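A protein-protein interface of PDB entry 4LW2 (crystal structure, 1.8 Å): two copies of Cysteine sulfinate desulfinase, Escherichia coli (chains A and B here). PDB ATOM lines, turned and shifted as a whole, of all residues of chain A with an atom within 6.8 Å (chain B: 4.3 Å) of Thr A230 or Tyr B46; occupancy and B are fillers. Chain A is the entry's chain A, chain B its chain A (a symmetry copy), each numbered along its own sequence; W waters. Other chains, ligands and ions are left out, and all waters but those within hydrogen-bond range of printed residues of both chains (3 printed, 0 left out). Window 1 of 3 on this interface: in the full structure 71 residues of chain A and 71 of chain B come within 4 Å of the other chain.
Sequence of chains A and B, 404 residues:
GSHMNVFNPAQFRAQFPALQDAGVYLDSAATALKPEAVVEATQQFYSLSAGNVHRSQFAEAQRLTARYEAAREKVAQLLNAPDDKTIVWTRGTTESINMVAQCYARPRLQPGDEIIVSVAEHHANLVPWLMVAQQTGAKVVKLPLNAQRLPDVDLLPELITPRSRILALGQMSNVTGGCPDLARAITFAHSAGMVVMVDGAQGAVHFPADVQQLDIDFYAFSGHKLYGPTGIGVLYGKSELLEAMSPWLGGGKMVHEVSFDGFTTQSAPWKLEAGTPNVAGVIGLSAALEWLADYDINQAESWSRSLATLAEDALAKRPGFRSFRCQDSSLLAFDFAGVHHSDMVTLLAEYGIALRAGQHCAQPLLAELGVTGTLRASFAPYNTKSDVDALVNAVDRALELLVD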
ATOM      1  N   PRO A  17      28.204  -3.673  36.819  1.00  0.00           N
ATOM      2  CA  PRO A  17      27.772  -4.632  37.832  1.00  0.00           C
ATOM      3  C   PRO A  17      28.879  -5.583  38.266  1.00  0.00           C
ATOM      4  O   PRO A  17      28.854  -6.091  39.389  1.00  0.00           O
ATOM      5  CB  PRO A  17      26.551  -5.326  37.149  1.00  0.00           C
ATOM      6  CG  PRO A  17      26.821  -5.206  35.629  1.00  0.00           C
ATOM      7  CD  PRO A  17      27.291  -3.653  35.679  1.00  0.00           C
ATOM      8  N   ALA A  18      29.917  -5.802  37.434  1.00  0.00           N
ATOM      9  CA  ALA A  18      30.893  -6.825  37.764  1.00  0.00           C
ATOM     10  C   ALA A  18      31.870  -6.377  38.839  1.00  0.00           C
ATOM     11  O   ALA A  18      32.613  -7.142  39.359  1.00  0.00           O
ATOM     12  CB  ALA A  18      31.739  -7.210  36.449  1.00  0.00           C
ATOM     13  N   THR A  31      40.319  -7.150  27.809  1.00  0.00           N
ATOM     14  CA  THR A  31      38.938  -6.990  27.490  1.00  0.00           C
ATOM     15  C   THR A  31      38.270  -6.127  28.591  1.00  0.00           C
ATOM     16  O   THR A  31      38.713  -6.196  29.727  1.00  0.00           O
ATOM     17  CB  THR A  31      38.236  -8.398  27.357  1.00  0.00           C
ATOM     18  OG1 THR A  31      37.056  -8.205  26.584  1.00  0.00           O
ATOM     19  CG2 THR A  31      37.921  -9.055  28.767  1.00  0.00           C
ATOM     20  N   LEU A  33      35.183  -4.512  31.189  1.00  0.00           N
ATOM     21  CA  LEU A  33      33.939  -4.888  31.886  1.00  0.00           C
ATOM     22  C   LEU A  33      32.806  -4.126  31.151  1.00  0.00           C
ATOM     23  O   LEU A  33      33.116  -3.191  30.372  1.00  0.00           O
ATOM     24  CB  LEU A  33      34.058  -4.400  33.337  1.00  0.00           C
ATOM     25  CG  LEU A  33      35.177  -5.135  34.160  1.00  0.00           C
ATOM     26  CD1 LEU A  33      35.211  -4.398  35.580  1.00  0.00           C
ATOM     27  CD2 LEU A  33      35.006  -6.663  34.162  1.00  0.00           C
ATOM     28  N   LYS A  34      31.534  -4.479  31.415  1.00  0.00           N
ATOM     29  CA  LYS A  34      30.452  -3.879  30.667  1.00  0.00           C
ATOM     30  C   LYS A  34      29.577  -3.041  31.555  1.00  0.00           C
ATOM     31  O   LYS A  34      29.268  -3.454  32.641  1.00  0.00           O
ATOM     32  CB  LYS A  34      29.554  -4.974  30.003  1.00  0.00           C
ATOM     33  CG  LYS A  34      30.346  -6.212  29.516  1.00  0.00           C
ATOM     34  CD  LYS A  34      31.274  -5.818  28.401  1.00  0.00           C
ATOM     35  CE  LYS A  34      32.128  -7.116  27.988  1.00  0.00           C
ATOM     36  NZ  LYS A  34      33.336  -6.746  27.087  1.00  0.00           N
ATOM     37  N   PRO A  35      29.055  -1.930  31.017  1.00  0.00           N
ATOM     38  CA  PRO A  35      28.119  -1.181  31.853  1.00  0.00           C
ATOM     39  C   PRO A  35      26.722  -1.875  31.849  1.00  0.00           C
ATOM     40  O   PRO A  35      26.412  -2.671  30.935  1.00  0.00           O
ATOM     41  CB  PRO A  35      27.972   0.119  31.085  1.00  0.00           C
ATOM     42  CG  PRO A  35      28.282  -0.199  29.581  1.00  0.00           C
ATOM     43  CD  PRO A  35      29.352  -1.295  29.700  1.00  0.00           C
ATOM     44  N   VAL A  38      24.616  -2.311  28.562  1.00  0.00           N
ATOM     45  CA  VAL A  38      24.994  -3.391  27.614  1.00  0.00           C
ATOM     46  C   VAL A  38      24.441  -4.709  28.135  1.00  0.00           C
ATOM     47  O   VAL A  38      23.856  -5.470  27.331  1.00  0.00           O
ATOM     48  CB  VAL A  38      26.519  -3.483  27.500  1.00  0.00           C
ATOM     49  CG1 VAL A  38      26.930  -4.768  26.766  1.00  0.00           C
ATOM     50  CG2 VAL A  38      27.037  -2.234  26.752  1.00  0.00           C
ATOM     51  N   VAL A  39      24.502  -4.915  29.464  1.00  0.00           N
ATOM     52  CA  VAL A  39      23.956  -6.144  30.025  1.00  0.00           C
ATOM     53  C   VAL A  39      22.429  -6.183  29.769  1.00  0.00           C
ATOM     54  O   VAL A  39      21.847  -7.190  29.329  1.00  0.00           O
ATOM     55  CB  VAL A  39      24.228  -6.226  31.531  1.00  0.00           C
ATOM     56  CG1 VAL A  39      23.562  -7.422  32.187  1.00  0.00           C
ATOM     57  CG2 VAL A  39      25.807  -6.199  31.874  1.00  0.00           C
ATOM     58  N   THR A  42      21.232  -6.557  26.057  1.00  0.00           N
ATOM     59  CA  THR A  42      21.444  -7.975  25.617  1.00  0.00           C
ATOM     60  C   THR A  42      20.398  -8.891  26.241  1.00  0.00           C
ATOM     61  O   THR A  42      19.859  -9.807  25.574  1.00  0.00           O
ATOM     62  CB  THR A  42      22.854  -8.429  26.050  1.00  0.00           C
ATOM     63  OG1 THR A  42      23.857  -7.552  25.496  1.00  0.00           O
ATOM     64  CG2 THR A  42      23.098  -9.856  25.622  1.00  0.00           C
ATOM     65  N   TYR A  46      17.591 -11.064  24.086  1.00  0.00           N
ATOM     66  CA  TYR A  46      17.376 -12.511  24.127  1.00  0.00           C
ATOM     67  C   TYR A  46      16.072 -12.970  24.852  1.00  0.00           C
ATOM     68  O   TYR A  46      15.729 -14.168  24.750  1.00  0.00           O
ATOM     69  CB  TYR A  46      18.604 -13.238  24.712  1.00  0.00           C
ATOM     70  CG  TYR A  46      19.833 -13.251  23.771  1.00  0.00           C
ATOM     71  CD1 TYR A  46      19.726 -13.782  22.477  1.00  0.00           C
ATOM     72  CD2 TYR A  46      21.108 -12.885  24.262  1.00  0.00           C
ATOM     73  CE1 TYR A  46      20.838 -13.871  21.601  1.00  0.00           C
ATOM     74  CE2 TYR A  46      22.236 -12.907  23.390  1.00  0.00           C
ATOM     75  CZ  TYR A  46      22.081 -13.431  22.094  1.00  0.00           C
ATOM     76  OH  TYR A  46      23.181 -13.513  21.301  1.00  0.00           O
ATOM     77  N   ARG A  91      33.544  -9.457  12.965  1.00  0.00           N
ATOM     78  CA  ARG A  91      33.536  -9.996  14.311  1.00  0.00           C
ATOM     79  C   ARG A  91      34.671  -9.487  15.173  1.00  0.00           C
ATOM     80  O   ARG A  91      34.779  -9.835  16.290  1.00  0.00           O
ATOM     81  CB  ARG A  91      33.582 -11.524  14.259  1.00  0.00           C
ATOM     82  CG  ARG A  91      34.866 -12.086  13.673  1.00  0.00           C
ATOM     83  CD  ARG A  91      34.893 -13.603  13.576  1.00  0.00           C
ATOM     84  NE  ARG A  91      36.155 -14.095  13.030  1.00  0.00           N
ATOM     85  CZ  ARG A  91      37.227 -14.367  13.760  1.00  0.00           C
ATOM     86  NH1 ARG A  91      37.196 -14.201  15.076  1.00  0.00           N
ATOM     87  NH2 ARG A  91      38.334 -14.811  13.178  1.00  0.00           N
ATOM     88  N   GLY A 223      34.531  -4.489  19.588  1.00  0.00           N
ATOM     89  CA  GLY A 223      33.527  -4.115  20.636  1.00  0.00           C
ATOM     90  C   GLY A 223      33.930  -4.486  22.052  1.00  0.00           C
ATOM     91  O   GLY A 223      33.647  -3.730  23.012  1.00  0.00           O
ATOM     92  N   HIS A 224      34.625  -5.619  22.219  1.00  0.00           N
ATOM     93  CA  HIS A 224      34.719  -6.162  23.587  1.00  0.00           C
ATOM     94  C   HIS A 224      35.699  -5.329  24.461  1.00  0.00           C
ATOM     95  O   HIS A 224      35.600  -5.282  25.689  1.00  0.00           O
ATOM     96  CB  HIS A 224      35.107  -7.663  23.525  1.00  0.00           C
ATOM     97  CG  HIS A 224      36.531  -7.928  23.106  1.00  0.00           C
ATOM     98  ND1 HIS A 224      36.910  -8.132  21.777  1.00  0.00           N
ATOM     99  CD2 HIS A 224      37.664  -8.052  23.854  1.00  0.00           C
ATOM    100  CE1 HIS A 224      38.226  -8.365  21.744  1.00  0.00           C
ATOM    101  NE2 HIS A 224      38.701  -8.347  22.975  1.00  0.00           N
ATOM    102  N   GLY A 228      31.977  -3.503  25.453  1.00  0.00           N
ATOM    103  CA  GLY A 228      30.815  -3.925  24.634  1.00  0.00           C
ATOM    104  C   GLY A 228      30.883  -5.443  24.389  1.00  0.00           C
ATOM    105  O   GLY A 228      31.711  -6.172  24.976  1.00  0.00           O
ATOM    106  N   PRO A 229      29.932  -5.930  23.606  1.00  0.00           N
ATOM    107  CA  PRO A 229      29.842  -7.437  23.403  1.00  0.00           C
ATOM    108  C   PRO A 229      31.110  -8.060  22.785  1.00  0.00           C
ATOM    109  O   PRO A 229      31.877  -7.378  22.033  1.00  0.00           O
ATOM    110  CB  PRO A 229      28.755  -7.554  22.340  1.00  0.00           C
ATOM    111  CG  PRO A 229      27.864  -6.321  22.554  1.00  0.00           C
ATOM    112  CD  PRO A 229      28.957  -5.199  22.813  1.00  0.00           C
ATOM    113  N   THR A 230      31.326  -9.372  23.032  1.00  0.00           N
ATOM    114  CA  THR A 230      32.253 -10.113  22.172  1.00  0.00           C
ATOM    115  C   THR A 230      31.646 -10.401  20.801  1.00  0.00           C
ATOM    116  O   THR A 230      30.418 -10.257  20.571  1.00  0.00           O
ATOM    117  CB  THR A 230      32.650 -11.472  22.832  1.00  0.00           C
ATOM    118  OG1 THR A 230      31.453 -12.244  23.147  1.00  0.00           O
ATOM    119  CG2 THR A 230      33.354 -11.242  24.174  1.00  0.00           C
ATOM    120  N   GLY A 231      32.507 -10.738  19.836  1.00  0.00           N
ATOM    121  CA  GLY A 231      32.031 -11.183  18.542  1.00  0.00           C
ATOM    122  C   GLY A 231      31.495 -10.067  17.671  1.00  0.00           C
ATOM    123  O   GLY A 231      30.747 -10.339  16.739  1.00  0.00           O
ATOM    124  N   ILE A 232      31.914  -8.837  17.934  1.00  0.00           N
ATOM    125  CA  ILE A 232      31.492  -7.728  17.075  1.00  0.00           C
ATOM    126  C   ILE A 232      32.642  -6.734  16.937  1.00  0.00           C
ATOM    127  O   ILE A 232      33.376  -6.430  17.907  1.00  0.00           O
ATOM    128  CB  ILE A 232      30.133  -7.044  17.647  1.00  0.00           C
ATOM    129  CG1 ILE A 232      29.535  -5.998  16.644  1.00  0.00           C
ATOM    130  CG2 ILE A 232      30.431  -6.302  18.999  1.00  0.00           C
ATOM    131  CD1 ILE A 232      29.228  -6.615  15.182  1.00  0.00           C
ATOM    132  N   GLY A 233      32.883  -6.233  15.707  1.00  0.00           N
ATOM    133  CA  GLY A 233      33.884  -5.185  15.578  1.00  0.00           C
ATOM    134  C   GLY A 233      33.450  -4.365  14.372  1.00  0.00           C
ATOM    135  O   GLY A 233      32.361  -4.564  13.831  1.00  0.00           O
ATOM    136  N   ASN A 278      25.467 -10.620  13.498  1.00  0.00           N
ATOM    137  CA  ASN A 278      25.482 -10.801  14.946  1.00  0.00           C
ATOM    138  C   ASN A 278      24.611  -9.727  15.598  1.00  0.00           C
ATOM    139  O   ASN A 278      25.116  -8.669  16.066  1.00  0.00           O
ATOM    140  CB  ASN A 278      26.885 -10.793  15.494  1.00  0.00           C
ATOM    141  CG  ASN A 278      26.887 -10.966  17.051  1.00  0.00           C
ATOM    142  OD1 ASN A 278      25.865 -11.328  17.629  1.00  0.00           O
ATOM    143  ND2 ASN A 278      28.049 -10.773  17.680  1.00  0.00           N
ATOM    144  N   ALA A 280      22.777  -9.568  18.281  1.00  0.00           N
ATOM    145  CA  ALA A 280      22.952  -9.252  19.723  1.00  0.00           C
ATOM    146  C   ALA A 280      24.217  -8.338  19.836  1.00  0.00           C
ATOM    147  O   ALA A 280      24.228  -7.388  20.653  1.00  0.00           O
ATOM    148  CB  ALA A 280      23.146 -10.534  20.604  1.00  0.00           C
ATOM    149  N   GLY A 281      25.303  -8.664  19.080  1.00  0.00           N
ATOM    150  CA  GLY A 281      26.497  -7.858  19.129  1.00  0.00           C
ATOM    151  C   GLY A 281      26.333  -6.432  18.632  1.00  0.00           C
ATOM    152  O   GLY A 281      26.852  -5.473  19.272  1.00  0.00           O
ATOM    153  N   THR B  42      24.247 -15.878  29.431  1.00  0.00           N
ATOM    154  CA  THR B  42      24.746 -14.629  28.767  1.00  0.00           C
ATOM    155  C   THR B  42      24.755 -13.467  29.752  1.00  0.00           C
ATOM    156  O   THR B  42      25.706 -12.649  29.779  1.00  0.00           O
ATOM    157  CB  THR B  42      23.825 -14.292  27.575  1.00  0.00           C
ATOM    158  OG1 THR B  42      23.777 -15.396  26.649  1.00  0.00           O
ATOM    159  CG2 THR B  42      24.301 -13.036  26.886  1.00  0.00           C
ATOM    160  N   GLN B  43      23.716 -13.354  30.566  1.00  0.00           N
ATOM    161  CA  GLN B  43      23.641 -12.303  31.604  1.00  0.00           C
ATOM    162  C   GLN B  43      24.774 -12.458  32.627  1.00  0.00           C
ATOM    163  O   GLN B  43      25.451 -11.479  32.961  1.00  0.00           O
ATOM    164  CB  GLN B  43      22.263 -12.445  32.314  1.00  0.00           C
ATOM    165  CG  GLN B  43      22.194 -11.696  33.712  1.00  0.00           C
ATOM    166  CD  GLN B  43      21.828 -10.331  33.457  1.00  0.00           C
ATOM    167  OE1 GLN B  43      21.504 -10.016  32.325  1.00  0.00           O
ATOM    168  NE2 GLN B  43      21.832  -9.464  34.501  1.00  0.00           N
ATOM    169  N   GLN B  44      25.043 -13.678  33.031  1.00  0.00           N
ATOM    170  CA  GLN B  44      26.166 -13.888  33.970  1.00  0.00           C
ATOM    171  C   GLN B  44      27.476 -13.531  33.260  1.00  0.00           C
ATOM    172  O   GLN B  44      28.313 -12.838  33.846  1.00  0.00           O
ATOM    173  CB  GLN B  44      26.181 -15.316  34.477  1.00  0.00           C
ATOM    174  CG  GLN B  44      24.998 -15.456  35.447  1.00  0.00           C
ATOM    175  CD  GLN B  44      25.087 -14.518  36.609  1.00  0.00           C
ATOM    176  OE1 GLN B  44      26.192 -14.060  36.955  1.00  0.00           O
ATOM    177  NE2 GLN B  44      23.949 -14.166  37.195  1.00  0.00           N
ATOM    178  N   PHE B  45      27.656 -14.026  32.045  1.00  0.00           N
ATOM    179  CA  PHE B  45      28.908 -13.753  31.352  1.00  0.00           C
ATOM    180  C   PHE B  45      29.194 -12.254  31.271  1.00  0.00           C
ATOM    181  O   PHE B  45      30.320 -11.811  31.492  1.00  0.00           O
ATOM    182  CB  PHE B  45      28.875 -14.325  29.942  1.00  0.00           C
ATOM    183  CG  PHE B  45      30.098 -13.923  29.155  1.00  0.00           C
ATOM    184  CD1 PHE B  45      31.337 -14.423  29.553  1.00  0.00           C
ATOM    185  CD2 PHE B  45      29.990 -13.009  28.140  1.00  0.00           C
ATOM    186  CE1 PHE B  45      32.560 -14.115  28.879  1.00  0.00           C
ATOM    187  CE2 PHE B  45      31.196 -12.629  27.383  1.00  0.00           C
ATOM    188  CZ  PHE B  45      32.502 -13.174  27.807  1.00  0.00           C
ATOM    189  N   TYR B  46      28.171 -11.438  30.962  1.00  0.00           N
ATOM    190  CA  TYR B  46      28.424 -10.000  30.862  1.00  0.00           C
ATOM    191  C   TYR B  46      28.389  -9.222  32.214  1.00  0.00           C
ATOM    192  O   TYR B  46      28.791  -8.038  32.227  1.00  0.00           O
ATOM    193  CB  TYR B  46      27.481  -9.341  29.835  1.00  0.00           C
ATOM    194  CG  TYR B  46      27.806  -9.699  28.364  1.00  0.00           C
ATOM    195  CD1 TYR B  46      29.084  -9.447  27.842  1.00  0.00           C
ATOM    196  CD2 TYR B  46      26.777 -10.123  27.492  1.00  0.00           C
ATOM    197  CE1 TYR B  46      29.411  -9.701  26.486  1.00  0.00           C
ATOM    198  CE2 TYR B  46      27.085 -10.443  26.137  1.00  0.00           C
ATOM    199  CZ  TYR B  46      28.383 -10.192  25.659  1.00  0.00           C
ATOM    200  OH  TYR B  46      28.640 -10.433  24.346  1.00  0.00           O
ATOM    201  N   SER B  47      27.959  -9.879  33.284  1.00  0.00           N
ATOM    202  CA  SER B  47      27.747  -9.237  34.613  1.00  0.00           C
ATOM    203  C   SER B  47      28.927  -9.574  35.551  1.00  0.00           C
ATOM    204  O   SER B  47      28.960  -9.107  36.702  1.00  0.00           O
ATOM    205  CB  SER B  47      26.398  -9.792  35.247  1.00  0.00           C
ATOM    206  OG  SER B  47      25.389  -9.076  34.549  1.00  0.00           O
ATOM    207  N   LEU B  48      29.876 -10.364  35.051  1.00  0.00           N
ATOM    208  CA  LEU B  48      31.056 -10.827  35.834  1.00  0.00           C
ATOM    209  C   LEU B  48      32.344 -10.582  35.058  1.00  0.00           C
ATOM    210  O   LEU B  48      32.437 -10.766  33.789  1.00  0.00           O
ATOM    211  CB  LEU B  48      30.938 -12.352  36.118  1.00  0.00           C
ATOM    212  CG  LEU B  48      29.753 -12.761  37.015  1.00  0.00           C
ATOM    213  CD1 LEU B  48      29.568 -14.335  37.092  1.00  0.00           C
ATOM    214  CD2 LEU B  48      29.780 -12.124  38.397  1.00  0.00           C
ATOM    215  N   PRO B 277      37.848 -14.966  20.469  1.00  0.00           N
ATOM    216  CA  PRO B 277      36.620 -15.661  20.054  1.00  0.00           C
ATOM    217  C   PRO B 277      35.408 -14.839  20.451  1.00  0.00           C
ATOM    218  O   PRO B 277      35.485 -13.987  21.335  1.00  0.00           O
ATOM    219  CB  PRO B 277      36.597 -16.918  20.958  1.00  0.00           C
ATOM    220  CG  PRO B 277      38.023 -17.108  21.494  1.00  0.00           C
ATOM    221  CD  PRO B 277      38.553 -15.647  21.573  1.00  0.00           C
ATOM    222  N   ASN B 278      34.266 -15.211  19.873  1.00  0.00           N
ATOM    223  CA  ASN B 278      32.987 -14.728  20.386  1.00  0.00           C
ATOM    224  C   ASN B 278      32.624 -15.508  21.650  1.00  0.00           C
ATOM    225  O   ASN B 278      31.845 -16.501  21.605  1.00  0.00           O
ATOM    226  CB  ASN B 278      31.902 -14.812  19.345  1.00  0.00           C
ATOM    227  CG  ASN B 278      30.530 -14.313  19.913  1.00  0.00           C
ATOM    228  OD1 ASN B 278      30.494 -13.699  20.977  1.00  0.00           O
ATOM    229  ND2 ASN B 278      29.449 -14.525  19.159  1.00  0.00           N
ATOM    230  N   VAL B 279      33.303 -15.161  22.729  1.00  0.00           N
ATOM    231  CA  VAL B 279      33.142 -15.895  23.999  1.00  0.00           C
ATOM    232  C   VAL B 279      31.701 -15.947  24.473  1.00  0.00           C
ATOM    233  O   VAL B 279      31.222 -17.032  24.890  1.00  0.00           O
ATOM    234  CB  VAL B 279      34.079 -15.351  25.155  1.00  0.00           C
ATOM    235  CG1 VAL B 279      33.887 -16.176  26.446  1.00  0.00           C
ATOM    236  CG2 VAL B 279      35.618 -15.403  24.647  1.00  0.00           C
ATOM    237  N   ALA B 280      30.973 -14.838  24.373  1.00  0.00           N
ATOM    238  CA  ALA B 280      29.564 -14.859  24.845  1.00  0.00           C
ATOM    239  C   ALA B 280      28.803 -15.893  23.951  1.00  0.00           C
ATOM    240  O   ALA B 280      27.936 -16.640  24.463  1.00  0.00           O
ATOM    241  CB  ALA B 280      28.870 -13.458  24.742  1.00  0.00           C
HETATM  242  O   HOH W   1      22.688  -9.897  29.443  1.00  0.00           O
HETATM  243  O   HOH W   2      35.199 -11.219  20.520  1.00  0.00           O
HETATM  244  O   HOH W   3      31.127  -6.900  32.981  1.00  0.00           O
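The side-chain hydroxyl of Thr A230 is in hydrogen-bond range of the backbone NH of Ala B280 (2.9 Å).
N of Thr A230 sits at hydrogen-bond distance from OH of Tyr B46, at 3.2 Å.
OD1 of Asn B278 lies within hydrogen-bond range of OG1 of Thr A230, at 2.8 Å.
N of Val B279 lies within hydrogen-bond range of OG1 of Thr A230, at 3.5 Å.
Water W3 lies within hydrogen-bond range of O of Tyr B46 (2.7 Å) and N of Lys A34 (2.9 Å).
Water W2 lies within hydrogen-bond range of the backbone NH (N) of Gly A231 (2.8 Å) and the backbone carbonyl oxygen (O) of Pro B277 (2.9 Å).
Water W1 lies within hydrogen-bond range of the backbone carbonyl oxygen of Val A39 (2.8 Å) and the side-chain amide oxygen of Gln B43 (3.1 Å).
Pro A17 touches Ser B47.
O of Ser B47 touches CA of Ala A18, at 3.2 Å.
CB of Ala A18 touches C of Leu B48, at 3.7 Å.
Lys A34 touches Tyr B46 (CG to O, 3.6 Å).
Val A39 touches Gln B43.
Val A39 touches Tyr B46.
CG1 of Val A39 touches OG of Ser B47, 3.4 Å away.
Thr B42 touches Thr A42 (CG2 to CG2, 3.6 Å).
Pro A229 touches Tyr B46 (CA to OH, 3.4 Å).
CA of Gly A231 touches CB of Asn B278, 3.7 Å away.
Thr B42 touches its own counterpart, Thr A42.
4 positions are printed for both chains.
Of the 11 printed residues of chain B, 8 touch a printed residue of chain A.
Printed residues of chain B that touch a printed residue of chain A: Thr B42, Gln B43, Tyr B46, Ser B47, Leu B48, Asn B278, Val B279 and Ala B280.
Hydrophobic or aromatic side chains of chain B that line the printed part of chain A: Tyr B46 and Ala B280.
Hydrophobic or aromatic side chains of chain A that line the printed part of chain B: Ala A18, Val A39 and Pro A229.
Val A38 touches none of the printed residues of chain B.
Printed residues of chain B within 4 Å of Pro A229: Tyr B46 (3.4 Å).
Of the printed residues of chain B, Thr A230 touches Tyr B46, Asn B278, Val B279 and Ala B280.
Gly A233 touches none of the printed residues of chain B.
Of the printed residues of chain A, Leu B48 touches Ala A18 (3.7 Å).
Of the printed residues of chain A, Ala B280 touches Thr A230.
The backbone carbonyl oxygen of Val A38 is in hydrogen-bond range of the side-chain hydroxyl of Thr A42 (2.8 Å).
The backbone carbonyl oxygen of Gln B43 is in hydrogen-bond range of the side-chain hydroxyl of Ser B47, at 2.9 Å.
The backbone carbonyl oxygen of Gly A228 lies within hydrogen-bond range of the side-chain amino group of Lys A34 (2.7 Å).
N of His A224 lies within hydrogen-bond range of O of Pro A229, at 3.3 Å.
O of Gly A231 sits at hydrogen-bond distance from ND2 of Asn A278, 2.9 Å away.
The backbone carbonyl oxygen (O) of His A224 lies within hydrogen-bond range of the side-chain amino group (NZ) of Lys A34 (3.0 Å).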
